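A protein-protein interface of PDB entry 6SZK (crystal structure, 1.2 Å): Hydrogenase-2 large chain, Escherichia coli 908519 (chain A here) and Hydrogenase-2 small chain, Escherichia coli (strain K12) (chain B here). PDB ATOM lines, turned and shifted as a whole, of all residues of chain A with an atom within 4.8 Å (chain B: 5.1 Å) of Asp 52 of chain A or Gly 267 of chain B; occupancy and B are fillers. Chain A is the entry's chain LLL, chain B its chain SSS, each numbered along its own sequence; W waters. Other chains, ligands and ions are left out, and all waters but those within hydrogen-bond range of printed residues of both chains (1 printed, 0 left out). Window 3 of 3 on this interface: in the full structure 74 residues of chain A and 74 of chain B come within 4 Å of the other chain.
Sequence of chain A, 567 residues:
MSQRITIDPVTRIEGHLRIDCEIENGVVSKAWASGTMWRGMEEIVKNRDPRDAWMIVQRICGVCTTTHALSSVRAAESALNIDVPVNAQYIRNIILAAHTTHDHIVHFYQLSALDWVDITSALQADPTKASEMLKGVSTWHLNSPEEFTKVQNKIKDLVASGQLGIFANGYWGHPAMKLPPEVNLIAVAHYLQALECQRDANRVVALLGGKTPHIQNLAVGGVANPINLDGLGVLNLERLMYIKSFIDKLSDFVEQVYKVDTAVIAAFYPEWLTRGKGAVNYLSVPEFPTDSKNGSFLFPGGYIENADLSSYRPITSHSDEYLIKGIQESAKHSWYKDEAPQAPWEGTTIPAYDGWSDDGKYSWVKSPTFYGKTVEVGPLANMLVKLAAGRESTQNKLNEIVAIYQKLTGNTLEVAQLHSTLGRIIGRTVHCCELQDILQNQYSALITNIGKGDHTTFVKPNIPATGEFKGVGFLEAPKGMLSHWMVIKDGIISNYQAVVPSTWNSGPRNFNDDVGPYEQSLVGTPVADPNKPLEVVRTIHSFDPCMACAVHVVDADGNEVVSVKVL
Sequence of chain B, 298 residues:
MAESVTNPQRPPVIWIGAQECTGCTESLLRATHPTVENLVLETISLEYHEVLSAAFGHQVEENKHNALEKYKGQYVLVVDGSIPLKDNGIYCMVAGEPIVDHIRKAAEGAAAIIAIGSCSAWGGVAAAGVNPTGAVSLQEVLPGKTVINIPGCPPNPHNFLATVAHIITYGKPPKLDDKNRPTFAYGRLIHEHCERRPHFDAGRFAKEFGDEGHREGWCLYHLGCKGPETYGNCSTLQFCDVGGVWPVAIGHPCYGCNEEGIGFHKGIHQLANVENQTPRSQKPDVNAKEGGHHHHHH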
ATOM      1  N   ASP A  49     -34.056 -13.875 -16.477  1.00  0.00           N
ATOM      2  CA  ASP A  49     -34.431 -13.493 -17.843  1.00  0.00           C
ATOM      3  C   ASP A  49     -33.437 -14.071 -18.865  1.00  0.00           C
ATOM      4  O   ASP A  49     -32.216 -13.949 -18.668  1.00  0.00           O
ATOM      5  CB  ASP A  49     -34.459 -11.971 -17.928  1.00  0.00           C
ATOM      6  CG  ASP A  49     -35.105 -11.453 -19.211  1.00  0.00           C
ATOM      7  OD1 ASP A  49     -34.619 -11.665 -20.315  1.00  0.00           O
ATOM      8  OD2 ASP A  49     -36.208 -10.829 -19.140  1.00  0.00           O
ATOM      9  N   PRO A  50     -33.907 -14.688 -19.968  1.00  0.00           N
ATOM     10  CA  PRO A  50     -32.999 -15.257 -20.978  1.00  0.00           C
ATOM     11  C   PRO A  50     -31.944 -14.261 -21.524  1.00  0.00           C
ATOM     12  O   PRO A  50     -30.831 -14.655 -21.903  1.00  0.00           O
ATOM     13  CB  PRO A  50     -33.945 -15.700 -22.119  1.00  0.00           C
ATOM     14  CG  PRO A  50     -35.178 -16.076 -21.344  1.00  0.00           C
ATOM     15  CD  PRO A  50     -35.312 -15.024 -20.279  1.00  0.00           C
ATOM     16  N   ARG A  51     -32.271 -12.953 -21.545  1.00  0.00           N
ATOM     17  CA  ARG A  51     -31.366 -11.903 -22.004  1.00  0.00           C
ATOM     18  C   ARG A  51     -30.118 -11.712 -21.130  1.00  0.00           C
ATOM     19  O   ARG A  51     -29.088 -11.190 -21.595  1.00  0.00           O
ATOM     20  CB  ARG A  51     -32.078 -10.556 -22.178  1.00  0.00           C
ATOM     21  CG  ARG A  51     -33.126 -10.583 -23.263  1.00  0.00           C
ATOM     22  CD  ARG A  51     -33.961  -9.331 -23.342  1.00  0.00           C
ATOM     23  NE  ARG A  51     -34.790  -9.216 -22.175  1.00  0.00           N
ATOM     24  CZ  ARG A  51     -35.272  -8.047 -21.718  1.00  0.00           C
ATOM     25  NH1 ARG A  51     -35.151  -6.907 -22.429  1.00  0.00           N
ATOM     26  NH2 ARG A  51     -35.988  -8.012 -20.582  1.00  0.00           N
ATOM     27  N   ASP A  52     -30.233 -12.082 -19.848  1.00  0.00           N
ATOM     28  CA  ASP A  52     -29.146 -11.852 -18.873  1.00  0.00           C
ATOM     29  C   ASP A  52     -28.091 -12.976 -18.902  1.00  0.00           C
ATOM     30  O   ASP A  52     -26.984 -12.796 -18.355  1.00  0.00           O
ATOM     31  CB  ASP A  52     -29.742 -11.714 -17.465  1.00  0.00           C
ATOM     32  CG  ASP A  52     -30.612 -10.458 -17.321  1.00  0.00           C
ATOM     33  OD1 ASP A  52     -30.324  -9.437 -17.964  1.00  0.00           O
ATOM     34  OD2 ASP A  52     -31.608 -10.444 -16.624  1.00  0.00           O
ATOM     35  N   ALA A  53     -28.441 -14.161 -19.465  1.00  0.00           N
ATOM     36  CA  ALA A  53     -27.574 -15.337 -19.291  1.00  0.00           C
ATOM     37  C   ALA A  53     -26.135 -15.109 -19.759  1.00  0.00           C
ATOM     38  O   ALA A  53     -25.173 -15.519 -19.069  1.00  0.00           O
ATOM     39  CB  ALA A  53     -28.158 -16.568 -19.948  1.00  0.00           C
ATOM     40  N   TRP A  54     -25.945 -14.448 -20.914  1.00  0.00           N
ATOM     41  CA  TRP A  54     -24.602 -14.392 -21.538  1.00  0.00           C
ATOM     42  C   TRP A  54     -23.579 -13.700 -20.647  1.00  0.00           C
ATOM     43  O   TRP A  54     -22.379 -14.101 -20.646  1.00  0.00           O
ATOM     44  CB  TRP A  54     -24.649 -13.783 -22.954  1.00  0.00           C
ATOM     45  CG  TRP A  54     -24.921 -12.275 -23.028  1.00  0.00           C
ATOM     46  CD1 TRP A  54     -26.159 -11.671 -23.143  1.00  0.00           C
ATOM     47  CD2 TRP A  54     -23.902 -11.255 -23.045  1.00  0.00           C
ATOM     48  NE1 TRP A  54     -25.975 -10.302 -23.256  1.00  0.00           N
ATOM     49  CE2 TRP A  54     -24.611 -10.016 -23.186  1.00  0.00           C
ATOM     50  CE3 TRP A  54     -22.517 -11.220 -22.927  1.00  0.00           C
ATOM     51  CZ2 TRP A  54     -23.944  -8.770 -23.203  1.00  0.00           C
ATOM     52  CZ3 TRP A  54     -21.847  -9.993 -23.001  1.00  0.00           C
ATOM     53  CH2 TRP A  54     -22.571  -8.791 -23.156  1.00  0.00           C
ATOM     54  N   MET A  55     -23.998 -12.648 -19.898  1.00  0.00           N
ATOM     55  CA  MET A  55     -23.042 -11.899 -19.053  1.00  0.00           C
ATOM     56  C   MET A  55     -22.580 -12.753 -17.856  1.00  0.00           C
ATOM     57  O   MET A  55     -21.478 -12.579 -17.332  1.00  0.00           O
ATOM     58  CB  MET A  55     -23.666 -10.571 -18.539  1.00  0.00           C
ATOM     59  CG  MET A  55     -23.446  -9.420 -19.565  1.00  0.00           C
ATOM     60  SD  MET A  55     -21.699  -8.886 -19.715  1.00  0.00           S
ATOM     61  CE  MET A  55     -21.516  -8.145 -18.107  1.00  0.00           C
ATOM     62  N   ILE A  56     -23.473 -13.676 -17.395  1.00  0.00           N
ATOM     63  CA  ILE A  56     -23.176 -14.552 -16.244  1.00  0.00           C
ATOM     64  C   ILE A  56     -22.332 -15.749 -16.712  1.00  0.00           C
ATOM     65  O   ILE A  56     -21.232 -16.023 -16.156  1.00  0.00           O
ATOM     66  CB  ILE A  56     -24.498 -14.999 -15.553  1.00  0.00           C
ATOM     67  CG1 ILE A  56     -25.149 -13.748 -14.892  1.00  0.00           C
ATOM     68  CG2 ILE A  56     -24.266 -16.135 -14.579  1.00  0.00           C
ATOM     69  CD1 ILE A  56     -26.654 -13.930 -14.595  1.00  0.00           C
ATOM     70  N   LYS B 226     -25.450   0.857 -14.996  1.00  0.00           N
ATOM     71  CA  LYS B 226     -25.230   0.834 -13.539  1.00  0.00           C
ATOM     72  C   LYS B 226     -24.151   1.816 -13.068  1.00  0.00           C
ATOM     73  O   LYS B 226     -23.795   1.845 -11.860  1.00  0.00           O
ATOM     74  CB  LYS B 226     -24.952  -0.581 -13.029  1.00  0.00           C
ATOM     75  CG  LYS B 226     -26.002  -1.620 -13.411  1.00  0.00           C
ATOM     76  CD  LYS B 226     -27.443  -1.247 -13.043  1.00  0.00           C
ATOM     77  CE  LYS B 226     -28.479  -2.366 -13.166  1.00  0.00           C
ATOM     78  NZ  LYS B 226     -28.457  -2.934 -14.582  1.00  0.00           N
ATOM     79  N   TYR B 255     -22.742  -2.892 -16.276  1.00  0.00           N
ATOM     80  CA  TYR B 255     -23.487  -3.960 -15.612  1.00  0.00           C
ATOM     81  C   TYR B 255     -23.264  -3.924 -14.096  1.00  0.00           C
ATOM     82  O   TYR B 255     -23.907  -4.736 -13.347  1.00  0.00           O
ATOM     83  CB  TYR B 255     -23.043  -5.293 -16.249  1.00  0.00           C
ATOM     84  CG  TYR B 255     -23.692  -6.561 -15.711  1.00  0.00           C
ATOM     85  CD1 TYR B 255     -24.994  -6.885 -15.992  1.00  0.00           C
ATOM     86  CD2 TYR B 255     -22.931  -7.527 -15.032  1.00  0.00           C
ATOM     87  CE1 TYR B 255     -25.557  -8.100 -15.588  1.00  0.00           C
ATOM     88  CE2 TYR B 255     -23.482  -8.790 -14.676  1.00  0.00           C
ATOM     89  CZ  TYR B 255     -24.814  -9.063 -14.922  1.00  0.00           C
ATOM     90  OH  TYR B 255     -25.298 -10.310 -14.541  1.00  0.00           O
ATOM     91  N   HIS B 265     -26.484  -9.689  -9.921  1.00  0.00           N
ATOM     92  CA  HIS B 265     -27.737  -9.653  -9.171  1.00  0.00           C
ATOM     93  C   HIS B 265     -28.835  -8.936  -9.944  1.00  0.00           C
ATOM     94  O   HIS B 265     -29.893  -9.534 -10.264  1.00  0.00           O
ATOM     95  CB  HIS B 265     -27.517  -9.023  -7.789  1.00  0.00           C
ATOM     96  CG  HIS B 265     -28.749  -8.970  -6.914  1.00  0.00           C
ATOM     97  ND1 HIS B 265     -29.429 -10.084  -6.433  1.00  0.00           N
ATOM     98  CD2 HIS B 265     -29.455  -7.895  -6.476  1.00  0.00           C
ATOM     99  CE1 HIS B 265     -30.485  -9.683  -5.711  1.00  0.00           C
ATOM    100  NE2 HIS B 265     -30.527  -8.377  -5.747  1.00  0.00           N
ATOM    101  N   LYS B 266     -28.591  -7.687 -10.306  1.00  0.00           N
ATOM    102  CA  LYS B 266     -29.559  -6.900 -11.114  1.00  0.00           C
ATOM    103  C   LYS B 266     -29.485  -7.331 -12.598  1.00  0.00           C
ATOM    104  O   LYS B 266     -28.395  -7.584 -13.157  1.00  0.00           O
ATOM    105  CB  LYS B 266     -29.288  -5.404 -10.950  1.00  0.00           C
ATOM    106  CG  LYS B 266     -29.538  -4.878  -9.544  1.00  0.00           C
ATOM    107  CD  LYS B 266     -29.537  -3.409  -9.453  1.00  0.00           C
ATOM    108  CE  LYS B 266     -29.709  -2.955  -8.023  1.00  0.00           C
ATOM    109  NZ  LYS B 266     -29.913  -1.483  -7.975  1.00  0.00           N
ATOM    110  N   GLY B 267     -30.644  -7.362 -13.277  1.00  0.00           N
ATOM    111  CA  GLY B 267     -30.674  -7.628 -14.718  1.00  0.00           C
ATOM    112  C   GLY B 267     -29.971  -6.570 -15.517  1.00  0.00           C
ATOM    113  O   GLY B 267     -29.891  -5.376 -15.100  1.00  0.00           O
ATOM    114  N   ILE B 268     -29.462  -6.931 -16.708  1.00  0.00           N
ATOM    115  CA  ILE B 268     -28.786  -5.982 -17.602  1.00  0.00           C
ATOM    116  C   ILE B 268     -29.667  -4.745 -17.792  1.00  0.00           C
ATOM    117  O   ILE B 268     -29.138  -3.583 -17.703  1.00  0.00           O
ATOM    118  CB  ILE B 268     -28.454  -6.609 -18.985  1.00  0.00           C
ATOM    119  CG1 ILE B 268     -27.411  -7.730 -18.933  1.00  0.00           C
ATOM    120  CG2 ILE B 268     -27.991  -5.488 -20.004  1.00  0.00           C
ATOM    121  CD1 ILE B 268     -27.190  -8.483 -20.230  1.00  0.00           C
ATOM    122  N   HIS B 269     -30.961  -4.954 -18.073  1.00  0.00           N
ATOM    123  CA  HIS B 269     -31.822  -3.817 -18.431  1.00  0.00           C
ATOM    124  C   HIS B 269     -32.616  -3.226 -17.266  1.00  0.00           C
ATOM    125  O   HIS B 269     -33.368  -2.245 -17.458  1.00  0.00           O
ATOM    126  CB  HIS B 269     -32.785  -4.264 -19.595  1.00  0.00           C
ATOM    127  CG  HIS B 269     -31.983  -4.634 -20.826  1.00  0.00           C
ATOM    128  ND1 HIS B 269     -31.016  -3.764 -21.416  1.00  0.00           N
ATOM    129  CD2 HIS B 269     -31.788  -5.799 -21.465  1.00  0.00           C
ATOM    130  CE1 HIS B 269     -30.465  -4.407 -22.491  1.00  0.00           C
ATOM    131  NE2 HIS B 269     -30.953  -5.653 -22.537  1.00  0.00           N
ATOM    132  N   GLN B 270     -32.413  -3.724 -16.039  1.00  0.00           N
ATOM    133  CA  GLN B 270     -32.967  -3.135 -14.841  1.00  0.00           C
ATOM    134  C   GLN B 270     -32.337  -1.761 -14.565  1.00  0.00           C
ATOM    135  O   GLN B 270     -31.130  -1.623 -14.723  1.00  0.00           O
ATOM    136  CB  GLN B 270     -32.724  -4.059 -13.673  1.00  0.00           C
ATOM    137  CG  GLN B 270     -33.294  -3.602 -12.319  1.00  0.00           C
ATOM    138  CD  GLN B 270     -33.091  -4.620 -11.192  1.00  0.00           C
ATOM    139  OE1 GLN B 270     -32.737  -5.818 -11.427  1.00  0.00           O
ATOM    140  NE2 GLN B 270     -33.210  -4.158  -9.938  1.00  0.00           N
HETATM  141  O   HOH W   1     -32.220  -7.509 -18.257  1.00  0.00           O
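The backbone NH (N) of Ile 268 of chain B sits at hydrogen-bond distance from the side-chain carboxylate (OD1) of Asp 52 of chain A (2.9 Å).
OE1 of Gln 270 of chain B lies within hydrogen-bond range of N of Gly 267 of chain B, at 3.2 Å. The side-chain carboxylate (OD1) of Asp 49 of chain A is in salt-bridge range of the guanidinium group (NE) of Arg 51 of chain A (3.1 Å). NZ of Lys 226 of chain B is in hydrogen-bond range of O of Ile 268 of chain B, 3.3 Å away. The side-chain amino group of Lys 226 of chain B is in hydrogen-bond range of the backbone carbonyl oxygen of Gly 267 of chain B (2.9 Å).
Among the printed residues, merely in contact across the chains: Arg 51 of chain A with Ile 268 of chain B, Arg 51 of chain A with His 269 of chain B, Asp 52 of chain A with Gly 267 of chain B, Trp 54 of chain A with Ile 268 of chain B, Met 55 of chain A with Tyr 255 of chain B, Met 55 of chain A with Ile 268 of chain B and Ile 56 of chain A with Tyr 255 of chain B.
Asp 52 of chain A touches just these residues of chain B: Gly 267 (3.5 Å) and Ile 268 (2.9 Å). Gly 267 of chain B touches just one residue of chain A: Asp 52. Printed residues of chain B within 4 Å of Ile 56 of chain A: Tyr 255. Of the printed residues of chain A, Ile 268 of chain B touches Arg 51, Asp 52, Trp 54 and Met 55. Printed residues of chain B within 4 Å of Trp 54 of chain A: Ile 268. Of the printed residues of chain A, Tyr 255 of chain B touches Met 55 (3.4 Å) and Ile 56 (3.5 Å). Printed residues of chain A within 4 Å of His 269 of chain B: Arg 51 (3.7 Å). Lys 266 of chain B touches none of the printed residues of chain A. The nearest printed residue of chain A that does not touch Gly 267 of chain B is Asp 49 of chain A (6.6 Å). The nearest printed residue of chain A that does not touch Tyr 255 of chain B is Asp 52 of chain A (4.9 Å).
Of the 8 printed residues of chain B, 4 touch a printed residue of chain A. Hydrophobic or aromatic side chains of chain B within 4 Å of the printed part of chain A: Tyr 255, Ile 268 and His 269. Along chain A the printed residues that touch a printed residue of chain B span positions 51 to 56. Among the printed residues, 8 pairs touch across the chains.
Water W1 lies within hydrogen-bond range of OD1 of Asp 52 of chain A, N of His 269 of chain B and N of Ile 268 of chain B.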
